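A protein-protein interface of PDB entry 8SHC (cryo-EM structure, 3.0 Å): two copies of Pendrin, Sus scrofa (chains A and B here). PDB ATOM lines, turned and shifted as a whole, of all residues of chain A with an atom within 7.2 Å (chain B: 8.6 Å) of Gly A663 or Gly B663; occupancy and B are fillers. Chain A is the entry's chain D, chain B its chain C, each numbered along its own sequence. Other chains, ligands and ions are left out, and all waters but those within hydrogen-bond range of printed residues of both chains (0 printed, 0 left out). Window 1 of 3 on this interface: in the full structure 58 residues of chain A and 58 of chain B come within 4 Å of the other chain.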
ATOM      1  N   ARG A 549     -13.366  10.980 -26.952  1.00  0.00           N
ATOM      2  CA  ARG A 549     -14.421  10.548 -26.045  1.00  0.00           C
ATOM      3  C   ARG A 549     -15.772  10.818 -26.690  1.00  0.00           C
ATOM      4  O   ARG A 549     -16.028  11.933 -27.155  1.00  0.00           O
ATOM      5  CB  ARG A 549     -14.327  11.265 -24.698  1.00  0.00           C
ATOM      6  CG  ARG A 549     -15.352  10.783 -23.689  1.00  0.00           C
ATOM      7  CD  ARG A 549     -15.193  11.462 -22.343  1.00  0.00           C
ATOM      8  NE  ARG A 549     -16.202  11.007 -21.394  1.00  0.00           N
ATOM      9  CZ  ARG A 549     -16.040   9.989 -20.559  1.00  0.00           C
ATOM     10  NH1 ARG A 549     -14.909   9.304 -20.515  1.00  0.00           N
ATOM     11  NH2 ARG A 549     -17.037   9.651 -19.746  1.00  0.00           N
ATOM     12  N   PHE A 550     -16.626   9.796 -26.714  1.00  0.00           N
ATOM     13  CA  PHE A 550     -17.963   9.855 -27.304  1.00  0.00           C
ATOM     14  C   PHE A 550     -18.950   9.434 -26.219  1.00  0.00           C
ATOM     15  O   PHE A 550     -19.212   8.240 -26.044  1.00  0.00           O
ATOM     16  CB  PHE A 550     -18.046   8.947 -28.529  1.00  0.00           C
ATOM     17  CG  PHE A 550     -19.347   9.036 -29.275  1.00  0.00           C
ATOM     18  CD1 PHE A 550     -19.608  10.102 -30.118  1.00  0.00           C
ATOM     19  CD2 PHE A 550     -20.303   8.042 -29.144  1.00  0.00           C
ATOM     20  CE1 PHE A 550     -20.801  10.180 -30.810  1.00  0.00           C
ATOM     21  CE2 PHE A 550     -21.498   8.115 -29.832  1.00  0.00           C
ATOM     22  CZ  PHE A 550     -21.747   9.184 -30.666  1.00  0.00           C
ATOM     23  N   SER A 551     -19.503  10.407 -25.489  1.00  0.00           N
ATOM     24  CA  SER A 551     -20.219  10.118 -24.246  1.00  0.00           C
ATOM     25  C   SER A 551     -21.665   9.727 -24.546  1.00  0.00           C
ATOM     26  O   SER A 551     -22.601  10.512 -24.384  1.00  0.00           O
ATOM     27  CB  SER A 551     -20.149  11.316 -23.307  1.00  0.00           C
ATOM     28  OG  SER A 551     -18.807  11.625 -22.974  1.00  0.00           O
ATOM     29  N   SER A 552     -21.842   8.478 -24.966  1.00  0.00           N
ATOM     30  CA  SER A 552     -23.162   7.912 -25.217  1.00  0.00           C
ATOM     31  C   SER A 552     -23.001   6.429 -25.536  1.00  0.00           C
ATOM     32  O   SER A 552     -21.912   5.991 -25.915  1.00  0.00           O
ATOM     33  CB  SER A 552     -23.868   8.619 -26.382  1.00  0.00           C
ATOM     34  OG  SER A 552     -25.266   8.393 -26.362  1.00  0.00           O
ATOM     35  N   LEU A 660      -9.728   5.356 -28.092  1.00  0.00           N
ATOM     36  CA  LEU A 660     -11.133   5.683 -27.884  1.00  0.00           C
ATOM     37  C   LEU A 660     -11.471   5.505 -26.410  1.00  0.00           C
ATOM     38  O   LEU A 660     -11.279   4.419 -25.853  1.00  0.00           O
ATOM     39  CB  LEU A 660     -12.035   4.803 -28.749  1.00  0.00           C
ATOM     40  CG  LEU A 660     -12.182   5.191 -30.221  1.00  0.00           C
ATOM     41  CD1 LEU A 660     -12.609   3.990 -31.048  1.00  0.00           C
ATOM     42  CD2 LEU A 660     -13.172   6.332 -30.379  1.00  0.00           C
ATOM     43  N   ASP A 661     -11.974   6.567 -25.785  1.00  0.00           N
ATOM     44  CA  ASP A 661     -12.417   6.517 -24.395  1.00  0.00           C
ATOM     45  C   ASP A 661     -13.899   6.158 -24.384  1.00  0.00           C
ATOM     46  O   ASP A 661     -14.739   6.947 -24.826  1.00  0.00           O
ATOM     47  CB  ASP A 661     -12.162   7.850 -23.696  1.00  0.00           C
ATOM     48  CG  ASP A 661     -12.565   7.828 -22.233  1.00  0.00           C
ATOM     49  OD1 ASP A 661     -12.621   6.727 -21.644  1.00  0.00           O
ATOM     50  OD2 ASP A 661     -12.820   8.912 -21.669  1.00  0.00           O
ATOM     51  N   CYS A 662     -14.217   4.970 -23.880  1.00  0.00           N
ATOM     52  CA  CYS A 662     -15.568   4.423 -23.923  1.00  0.00           C
ATOM     53  C   CYS A 662     -16.127   4.219 -22.521  1.00  0.00           C
ATOM     54  O   CYS A 662     -16.825   3.240 -22.248  1.00  0.00           O
ATOM     55  CB  CYS A 662     -15.594   3.116 -24.709  1.00  0.00           C
ATOM     56  SG  CYS A 662     -14.719   3.171 -26.289  1.00  0.00           S
ATOM     57  N   GLY A 663     -15.827   5.147 -21.612  1.00  0.00           N
ATOM     58  CA  GLY A 663     -16.337   5.032 -20.257  1.00  0.00           C
ATOM     59  C   GLY A 663     -17.829   5.270 -20.153  1.00  0.00           C
ATOM     60  O   GLY A 663     -18.473   4.792 -19.214  1.00  0.00           O
ATOM     61  N   ALA A 664     -18.402   6.003 -21.106  1.00  0.00           N
ATOM     62  CA  ALA A 664     -19.812   6.366 -21.079  1.00  0.00           C
ATOM     63  C   ALA A 664     -20.663   5.536 -22.032  1.00  0.00           C
ATOM     64  O   ALA A 664     -21.843   5.846 -22.217  1.00  0.00           O
ATOM     65  CB  ALA A 664     -19.978   7.853 -21.395  1.00  0.00           C
ATOM     66  N   VAL A 665     -20.098   4.497 -22.641  1.00  0.00           N
ATOM     67  CA  VAL A 665     -20.851   3.635 -23.547  1.00  0.00           C
ATOM     68  C   VAL A 665     -21.689   2.680 -22.703  1.00  0.00           C
ATOM     69  O   VAL A 665     -21.156   1.780 -22.051  1.00  0.00           O
ATOM     70  CB  VAL A 665     -19.926   2.870 -24.500  1.00  0.00           C
ATOM     71  CG1 VAL A 665     -20.737   1.964 -25.411  1.00  0.00           C
ATOM     72  CG2 VAL A 665     -19.094   3.843 -25.318  1.00  0.00           C
ATOM     73  N   SER A 666     -23.008   2.878 -22.712  1.00  0.00           N
ATOM     74  CA  SER A 666     -23.894   2.095 -21.856  1.00  0.00           C
ATOM     75  C   SER A 666     -24.195   0.727 -22.461  1.00  0.00           C
ATOM     76  O   SER A 666     -23.876  -0.309 -21.868  1.00  0.00           O
ATOM     77  CB  SER A 666     -25.190   2.868 -21.599  1.00  0.00           C
ATOM     78  OG  SER A 666     -24.921   4.189 -21.165  1.00  0.00           O
ATOM     79  N   ALA A 693     -10.415   1.717 -24.395  1.00  0.00           N
ATOM     80  CA  ALA A 693     -10.128   1.843 -22.976  1.00  0.00           C
ATOM     81  C   ALA A 693     -11.398   2.197 -22.218  1.00  0.00           C
ATOM     82  O   ALA A 693     -12.315   2.818 -22.765  1.00  0.00           O
ATOM     83  CB  ALA A 693      -9.045   2.898 -22.713  1.00  0.00           C
ATOM     84  N   SER A 694     -11.443   1.779 -20.952  1.00  0.00           N
ATOM     85  CA  SER A 694     -12.542   2.085 -20.034  1.00  0.00           C
ATOM     86  C   SER A 694     -13.871   1.492 -20.498  1.00  0.00           C
ATOM     87  O   SER A 694     -14.935   2.058 -20.240  1.00  0.00           O
ATOM     88  CB  SER A 694     -12.681   3.594 -19.815  1.00  0.00           C
ATOM     89  OG  SER A 694     -11.565   4.109 -19.111  1.00  0.00           O
ATOM     90  N   LEU A 695     -13.826   0.354 -21.185  1.00  0.00           N
ATOM     91  CA  LEU A 695     -15.049  -0.320 -21.596  1.00  0.00           C
ATOM     92  C   LEU A 695     -15.583  -1.189 -20.462  1.00  0.00           C
ATOM     93  O   LEU A 695     -14.830  -1.941 -19.835  1.00  0.00           O
ATOM     94  CB  LEU A 695     -14.796  -1.165 -22.843  1.00  0.00           C
ATOM     95  CG  LEU A 695     -15.201  -0.508 -24.165  1.00  0.00           C
ATOM     96  CD1 LEU A 695     -14.744  -1.331 -25.357  1.00  0.00           C
ATOM     97  CD2 LEU A 695     -16.706  -0.305 -24.204  1.00  0.00           C
ATOM     98  N   GLN A 696     -16.884  -1.088 -20.205  1.00  0.00           N
ATOM     99  CA  GLN A 696     -17.503  -1.883 -19.156  1.00  0.00           C
ATOM    100  C   GLN A 696     -17.545  -3.353 -19.556  1.00  0.00           C
ATOM    101  O   GLN A 696     -17.431  -3.706 -20.733  1.00  0.00           O
ATOM    102  CB  GLN A 696     -18.912  -1.375 -18.856  1.00  0.00           C
ATOM    103  CG  GLN A 696     -18.916  -0.159 -17.958  1.00  0.00           C
ATOM    104  CD  GLN A 696     -18.204  -0.424 -16.657  1.00  0.00           C
ATOM    105  OE1 GLN A 696     -17.076   0.021 -16.456  1.00  0.00           O
ATOM    106  NE2 GLN A 696     -18.849  -1.170 -15.769  1.00  0.00           N
ATOM    107  N   LEU B 521     -19.350  -1.739  -6.050  1.00  0.00           N
ATOM    108  CA  LEU B 521     -17.946  -1.872  -6.410  1.00  0.00           C
ATOM    109  C   LEU B 521     -17.046  -1.936  -5.182  1.00  0.00           C
ATOM    110  O   LEU B 521     -17.328  -1.336  -4.142  1.00  0.00           O
ATOM    111  CB  LEU B 521     -17.508  -0.710  -7.304  1.00  0.00           C
ATOM    112  CG  LEU B 521     -18.407  -0.403  -8.502  1.00  0.00           C
ATOM    113  CD1 LEU B 521     -17.907   0.822  -9.248  1.00  0.00           C
ATOM    114  CD2 LEU B 521     -18.490  -1.603  -9.430  1.00  0.00           C
ATOM    115  N   LEU B 548     -21.574   2.607  -5.468  1.00  0.00           N
ATOM    116  CA  LEU B 548     -22.613   2.185  -6.397  1.00  0.00           C
ATOM    117  C   LEU B 548     -22.357   2.796  -7.766  1.00  0.00           C
ATOM    118  O   LEU B 548     -22.096   3.999  -7.874  1.00  0.00           O
ATOM    119  CB  LEU B 548     -24.002   2.585  -5.891  1.00  0.00           C
ATOM    120  CG  LEU B 548     -25.178   2.207  -6.797  1.00  0.00           C
ATOM    121  CD1 LEU B 548     -25.694   0.820  -6.455  1.00  0.00           C
ATOM    122  CD2 LEU B 548     -26.294   3.233  -6.704  1.00  0.00           C
ATOM    123  N   ARG B 549     -22.434   1.968  -8.802  1.00  0.00           N
ATOM    124  CA  ARG B 549     -22.348   2.416 -10.184  1.00  0.00           C
ATOM    125  C   ARG B 549     -23.691   2.192 -10.863  1.00  0.00           C
ATOM    126  O   ARG B 549     -24.246   1.092 -10.795  1.00  0.00           O
ATOM    127  CB  ARG B 549     -21.244   1.677 -10.943  1.00  0.00           C
ATOM    128  CG  ARG B 549     -21.059   2.175 -12.366  1.00  0.00           C
ATOM    129  CD  ARG B 549     -19.915   1.474 -13.071  1.00  0.00           C
ATOM    130  NE  ARG B 549     -19.767   1.945 -14.443  1.00  0.00           N
ATOM    131  CZ  ARG B 549     -18.981   2.946 -14.812  1.00  0.00           C
ATOM    132  NH1 ARG B 549     -18.237   3.600 -13.934  1.00  0.00           N
ATOM    133  NH2 ARG B 549     -18.938   3.301 -16.092  1.00  0.00           N
ATOM    134  N   PHE B 550     -24.203   3.237 -11.511  1.00  0.00           N
ATOM    135  CA  PHE B 550     -25.488   3.223 -12.209  1.00  0.00           C
ATOM    136  C   PHE B 550     -25.222   3.656 -13.648  1.00  0.00           C
ATOM    137  O   PHE B 550     -25.209   4.854 -13.947  1.00  0.00           O
ATOM    138  CB  PHE B 550     -26.484   4.150 -11.513  1.00  0.00           C
ATOM    139  CG  PHE B 550     -27.871   4.106 -12.086  1.00  0.00           C
ATOM    140  CD1 PHE B 550     -28.726   3.057 -11.793  1.00  0.00           C
ATOM    141  CD2 PHE B 550     -28.326   5.124 -12.908  1.00  0.00           C
ATOM    142  CE1 PHE B 550     -30.004   3.020 -12.316  1.00  0.00           C
ATOM    143  CE2 PHE B 550     -29.603   5.093 -13.433  1.00  0.00           C
ATOM    144  CZ  PHE B 550     -30.443   4.041 -13.136  1.00  0.00           C
ATOM    145  N   SER B 551     -25.009   2.688 -14.545  1.00  0.00           N
ATOM    146  CA  SER B 551     -24.454   2.980 -15.867  1.00  0.00           C
ATOM    147  C   SER B 551     -25.565   3.415 -16.822  1.00  0.00           C
ATOM    148  O   SER B 551     -26.031   2.655 -17.674  1.00  0.00           O
ATOM    149  CB  SER B 551     -23.702   1.769 -16.402  1.00  0.00           C
ATOM    150  OG  SER B 551     -22.626   1.420 -15.549  1.00  0.00           O
ATOM    151  N   SER B 552     -25.972   4.673 -16.689  1.00  0.00           N
ATOM    152  CA  SER B 552     -26.960   5.280 -17.572  1.00  0.00           C
ATOM    153  C   SER B 552     -27.074   6.760 -17.231  1.00  0.00           C
ATOM    154  O   SER B 552     -26.696   7.175 -16.131  1.00  0.00           O
ATOM    155  CB  SER B 552     -28.333   4.608 -17.428  1.00  0.00           C
ATOM    156  OG  SER B 552     -29.165   4.873 -18.543  1.00  0.00           O
ATOM    157  N   PRO B 553     -27.590   7.569 -18.157  1.00  0.00           N
ATOM    158  CA  PRO B 553     -28.065   8.905 -17.783  1.00  0.00           C
ATOM    159  C   PRO B 553     -29.258   8.798 -16.844  1.00  0.00           C
ATOM    160  O   PRO B 553     -29.878   7.742 -16.703  1.00  0.00           O
ATOM    161  CB  PRO B 553     -28.462   9.536 -19.125  1.00  0.00           C
ATOM    162  CG  PRO B 553     -28.592   8.386 -20.075  1.00  0.00           C
ATOM    163  CD  PRO B 553     -27.600   7.372 -19.615  1.00  0.00           C
ATOM    164  N   LEU B 660     -20.958   7.508  -5.152  1.00  0.00           N
ATOM    165  CA  LEU B 660     -21.661   7.216  -6.395  1.00  0.00           C
ATOM    166  C   LEU B 660     -20.696   7.383  -7.561  1.00  0.00           C
ATOM    167  O   LEU B 660     -20.110   8.456  -7.736  1.00  0.00           O
ATOM    168  CB  LEU B 660     -22.872   8.131  -6.568  1.00  0.00           C
ATOM    169  CG  LEU B 660     -24.138   7.767  -5.789  1.00  0.00           C
ATOM    170  CD1 LEU B 660     -25.020   8.989  -5.605  1.00  0.00           C
ATOM    171  CD2 LEU B 660     -24.899   6.656  -6.491  1.00  0.00           C
ATOM    172  N   ASP B 661     -20.537   6.326  -8.356  1.00  0.00           N
ATOM    173  CA  ASP B 661     -19.708   6.370  -9.555  1.00  0.00           C
ATOM    174  C   ASP B 661     -20.594   6.768 -10.729  1.00  0.00           C
ATOM    175  O   ASP B 661     -21.479   6.008 -11.135  1.00  0.00           O
ATOM    176  CB  ASP B 661     -19.034   5.022  -9.798  1.00  0.00           C
ATOM    177  CG  ASP B 661     -18.122   5.035 -11.011  1.00  0.00           C
ATOM    178  OD1 ASP B 661     -17.662   6.128 -11.401  1.00  0.00           O
ATOM    179  OD2 ASP B 661     -17.863   3.951 -11.572  1.00  0.00           O
ATOM    180  N   CYS B 662     -20.358   7.958 -11.274  1.00  0.00           N
ATOM    181  CA  CYS B 662     -21.202   8.541 -12.308  1.00  0.00           C
ATOM    182  C   CYS B 662     -20.430   8.743 -13.606  1.00  0.00           C
ATOM    183  O   CYS B 662     -20.614   9.737 -14.312  1.00  0.00           O
ATOM    184  CB  CYS B 662     -21.805   9.860 -11.831  1.00  0.00           C
ATOM    185  SG  CYS B 662     -22.519   9.802 -10.173  1.00  0.00           S
ATOM    186  N   GLY B 663     -19.552   7.795 -13.937  1.00  0.00           N
ATOM    187  CA  GLY B 663     -18.789   7.906 -15.167  1.00  0.00           C
ATOM    188  C   GLY B 663     -19.624   7.707 -16.414  1.00  0.00           C
ATOM    189  O   GLY B 663     -19.262   8.190 -17.490  1.00  0.00           O
ATOM    190  N   ALA B 664     -20.748   7.003 -16.295  1.00  0.00           N
ATOM    191  CA  ALA B 664     -21.598   6.678 -17.432  1.00  0.00           C
ATOM    192  C   ALA B 664     -22.849   7.543 -17.511  1.00  0.00           C
ATOM    193  O   ALA B 664     -23.725   7.269 -18.336  1.00  0.00           O
ATOM    194  CB  ALA B 664     -21.990   5.201 -17.390  1.00  0.00           C
ATOM    195  N   VAL B 665     -22.958   8.575 -16.678  1.00  0.00           N
ATOM    196  CA  VAL B 665     -24.111   9.470 -16.708  1.00  0.00           C
ATOM    197  C   VAL B 665     -23.929  10.436 -17.875  1.00  0.00           C
ATOM    198  O   VAL B 665     -23.063  11.312 -17.839  1.00  0.00           O
ATOM    199  CB  VAL B 665     -24.279  10.221 -15.383  1.00  0.00           C
ATOM    200  CG1 VAL B 665     -25.471  11.162 -15.456  1.00  0.00           C
ATOM    201  CG2 VAL B 665     -24.445   9.236 -14.238  1.00  0.00           C
ATOM    202  N   SER B 666     -24.748  10.273 -18.915  1.00  0.00           N
ATOM    203  CA  SER B 666     -24.590  11.070 -20.128  1.00  0.00           C
ATOM    204  C   SER B 666     -25.216  12.453 -19.978  1.00  0.00           C
ATOM    205  O   SER B 666     -24.523  13.472 -20.074  1.00  0.00           O
ATOM    206  CB  SER B 666     -25.200  10.329 -21.321  1.00  0.00           C
ATOM    207  OG  SER B 666     -24.729   8.995 -21.392  1.00  0.00           O
ATOM    208  N   PHE B 692     -19.834  12.258  -4.878  1.00  0.00           N
ATOM    209  CA  PHE B 692     -19.942  11.998  -6.305  1.00  0.00           C
ATOM    210  C   PHE B 692     -18.551  11.983  -6.919  1.00  0.00           C
ATOM    211  O   PHE B 692     -17.672  12.745  -6.505  1.00  0.00           O
ATOM    212  CB  PHE B 692     -20.809  13.052  -6.998  1.00  0.00           C
ATOM    213  CG  PHE B 692     -22.204  13.146  -6.451  1.00  0.00           C
ATOM    214  CD1 PHE B 692     -22.494  14.005  -5.404  1.00  0.00           C
ATOM    215  CD2 PHE B 692     -23.224  12.377  -6.983  1.00  0.00           C
ATOM    216  CE1 PHE B 692     -23.776  14.094  -4.899  1.00  0.00           C
ATOM    217  CE2 PHE B 692     -24.508  12.462  -6.482  1.00  0.00           C
ATOM    218  CZ  PHE B 692     -24.784  13.322  -5.438  1.00  0.00           C
ATOM    219  N   ALA B 693     -18.355  11.113  -7.908  1.00  0.00           N
ATOM    220  CA  ALA B 693     -17.060  10.960  -8.549  1.00  0.00           C
ATOM    221  C   ALA B 693     -17.247  10.631 -10.022  1.00  0.00           C
ATOM    222  O   ALA B 693     -18.255  10.042 -10.421  1.00  0.00           O
ATOM    223  CB  ALA B 693     -16.220   9.872  -7.867  1.00  0.00           C
ATOM    224  N   SER B 694     -16.260  11.033 -10.827  1.00  0.00           N
ATOM    225  CA  SER B 694     -16.213  10.745 -12.262  1.00  0.00           C
ATOM    226  C   SER B 694     -17.376  11.378 -13.021  1.00  0.00           C
ATOM    227  O   SER B 694     -17.835  10.838 -14.030  1.00  0.00           O
ATOM    228  CB  SER B 694     -16.165   9.237 -12.525  1.00  0.00           C
ATOM    229  OG  SER B 694     -14.940   8.683 -12.078  1.00  0.00           O
ATOM    230  N   LEU B 695     -17.862  12.524 -12.549  1.00  0.00           N
ATOM    231  CA  LEU B 695     -18.918  13.235 -13.258  1.00  0.00           C
ATOM    232  C   LEU B 695     -18.325  14.102 -14.362  1.00  0.00           C
ATOM    233  O   LEU B 695     -17.348  14.827 -14.143  1.00  0.00           O
ATOM    234  CB  LEU B 695     -19.727  14.090 -12.284  1.00  0.00           C
ATOM    235  CG  LEU B 695     -21.038  13.465 -11.803  1.00  0.00           C
ATOM    236  CD1 LEU B 695     -21.678  14.293 -10.702  1.00  0.00           C
ATOM    237  CD2 LEU B 695     -21.995  13.300 -12.971  1.00  0.00           C
ATOM    238  N   GLN B 696     -18.920  14.031 -15.550  1.00  0.00           N
ATOM    239  CA  GLN B 696     -18.449  14.828 -16.671  1.00  0.00           C
ATOM    240  C   GLN B 696     -18.755  16.303 -16.441  1.00  0.00           C
ATOM    241  O   GLN B 696     -19.605  16.666 -15.622  1.00  0.00           O
ATOM    242  CB  GLN B 696     -19.086  14.353 -17.975  1.00  0.00           C
ATOM    243  CG  GLN B 696     -18.408  13.127 -18.544  1.00  0.00           C
ATOM    244  CD  GLN B 696     -16.937  13.358 -18.772  1.00  0.00           C
ATOM    245  OE1 GLN B 696     -16.100  12.879 -18.008  1.00  0.00           O
ATOM    246  NE2 GLN B 696     -16.608  14.108 -19.816  1.00  0.00           N
ATOM    247  N   HIS B 698     -20.051  18.804 -18.547  1.00  0.00           N
ATOM    248  CA  HIS B 698     -21.326  19.351 -19.007  1.00  0.00           C
ATOM    249  C   HIS B 698     -22.462  18.979 -18.066  1.00  0.00           C
ATOM    250  O   HIS B 698     -23.375  19.783 -17.840  1.00  0.00           O
ATOM    251  CB  HIS B 698     -21.620  18.875 -20.429  1.00  0.00           C
ATOM    252  CG  HIS B 698     -21.628  17.385 -20.584  1.00  0.00           C
ATOM    253  ND1 HIS B 698     -20.473  16.640 -20.686  1.00  0.00           N
ATOM    254  CD2 HIS B 698     -22.653  16.504 -20.675  1.00  0.00           C
ATOM    255  CE1 HIS B 698     -20.785  15.363 -20.819  1.00  0.00           C
ATOM    256  NE2 HIS B 698     -22.100  15.254 -20.817  1.00  0.00           N
ATOM    257  N   VAL B 699     -22.395  17.789 -17.468  1.00  0.00           N
ATOM    258  CA  VAL B 699     -23.330  17.434 -16.408  1.00  0.00           C
ATOM    259  C   VAL B 699     -23.147  18.357 -15.208  1.00  0.00           C
ATOM    260  O   VAL B 699     -24.114  18.692 -14.513  1.00  0.00           O
ATOM    261  CB  VAL B 699     -23.157  15.954 -16.021  1.00  0.00           C
ATOM    262  CG1 VAL B 699     -24.143  15.562 -14.933  1.00  0.00           C
ATOM    263  CG2 VAL B 699     -23.315  15.069 -17.247  1.00  0.00           C
ATOM    264  N   LEU B 720     -12.607  13.500  -8.772  1.00  0.00           N
ATOM    265  CA  LEU B 720     -12.308  13.194 -10.169  1.00  0.00           C
ATOM    266  C   LEU B 720     -12.579  11.730 -10.503  1.00  0.00           C
ATOM    267  O   LEU B 720     -13.210  11.426 -11.521  1.00  0.00           O
ATOM    268  CB  LEU B 720     -10.855  13.552 -10.479  1.00  0.00           C
ATOM    269  CG  LEU B 720     -10.451  15.010 -10.243  1.00  0.00           C
ATOM    270  CD1 LEU B 720      -9.033  15.257 -10.728  1.00  0.00           C
ATOM    271  CD2 LEU B 720     -11.424  15.963 -10.920  1.00  0.00           C
ATOM    272  N   THR B 721     -12.098  10.811  -9.667  1.00  0.00           N
ATOM    273  CA  THR B 721     -12.282   9.379  -9.865  1.00  0.00           C
ATOM    274  C   THR B 721     -12.586   8.746  -8.517  1.00  0.00           C
ATOM    275  O   THR B 721     -12.447   9.384  -7.469  1.00  0.00           O
ATOM    276  CB  THR B 721     -11.043   8.716 -10.487  1.00  0.00           C
ATOM    277  OG1 THR B 721      -9.922   8.877  -9.609  1.00  0.00           O
ATOM    278  CG2 THR B 721     -10.716   9.317 -11.847  1.00  0.00           C
ATOM    279  N   VAL B 722     -13.009   7.481  -8.531  1.00  0.00           N
ATOM    280  CA  VAL B 722     -13.201   6.813  -7.250  1.00  0.00           C
ATOM    281  C   VAL B 722     -11.890   6.154  -6.848  1.00  0.00           C
ATOM    282  O   VAL B 722     -11.762   4.925  -6.852  1.00  0.00           O
ATOM    283  CB  VAL B 722     -14.336   5.776  -7.320  1.00  0.00           C
ATOM    284  CG1 VAL B 722     -14.749   5.337  -5.921  1.00  0.00           C
ATOM    285  CG2 VAL B 722     -15.524   6.331  -8.090  1.00  0.00           C
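The backbone carbonyl oxygen of Gly A663 is in hydrogen-bond range of the guanidinium group of Arg B549 (3.5 Å).
O of Gly B663 is in hydrogen-bond range of NH2 of Arg A549 (3.5 Å).
Arg A549 touches Gly B663, and with the chains exchanged Gly A663 touches Arg B549.
Arg A549 touches Gln B696, and with the chains exchanged Gln A696 touches Arg B549.
Ser A551 touches Ser B666, and with the chains exchanged Ser A666 touches Ser B551.
Gly A663 touches its own counterpart, Gly B663.
Of the 9 pairs that touch across the chains among the printed residues, 9 have their exchanged pair printed and touching as well.
Among the printed residues, merely in contact across the chains: Arg A549 with Gln B696 (3.5 Å), Gln A696 with Arg B549 (3.5 Å), Gly A663 with Gly B663 (3.9 Å), Ser A666 with Ser B551 (3.97 Å), Ser A551 with Ser B666 (3.97 Å), Gly A663 with Ala B664 (3.98 Å) and Ala A664 with Gly B663 (3.98 Å).
Of the printed residues of chain B, Gly A663 touches Arg B549, Gly B663 and Ala B664.
Printed residues of chain B within 4 Å of Gln A696: Arg B549 (3.5 Å).
Of the printed residues of chain A, Gly B663 touches Arg A549, Gly A663 and Ala A664.
Printed residues of chain A within 4 Å of Gln B696: Arg A549 (3.5 Å).
The nearest printed residue of chain B that does not touch Gly A663 is Val B665 (6.4 Å).
The nearest printed residue of chain A that does not touch Gly B663 is Val A665 (6.4 Å).
The nearest printed residue of chain B that does not touch Ser A666 is Ser B552 (4.3 Å).
The guanidinium group of Arg B549 lies within salt-bridge range of the side-chain carboxylate of Asp B661 (2.4 Å).
The guanidinium group of Arg B549 sits at hydrogen-bond distance from the side-chain hydroxyl of Ser B551 (3.1 Å).
The side-chain carboxylate of Asp A661 is in salt-bridge range of the guanidinium group of Arg A549 (2.4 Å).
The guanidinium group (NE) of Arg A549 sits at hydrogen-bond distance from the side-chain hydroxyl (OG) of Ser A551 (3.1 Å).
N of Gly A663 lies close to O of Ser A694 (3.5 Å).
The backbone NH of Gly B663 lies close to the backbone carbonyl oxygen of Ser B694 (3.5 Å).
Of the 24 printed residues of chain B, 6 touch a printed residue of chain A.
Hydrophobic or aromatic side chains of chain B that line the printed part of chain A: Ala B664.
Hydrophobic or aromatic side chains of chain A that line the printed part of chain B: Ala A664.
Among the printed residues, no Asp or Glu carboxylate lies within 4 Å of a Lys or Arg side-chain nitrogen of the other chain.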
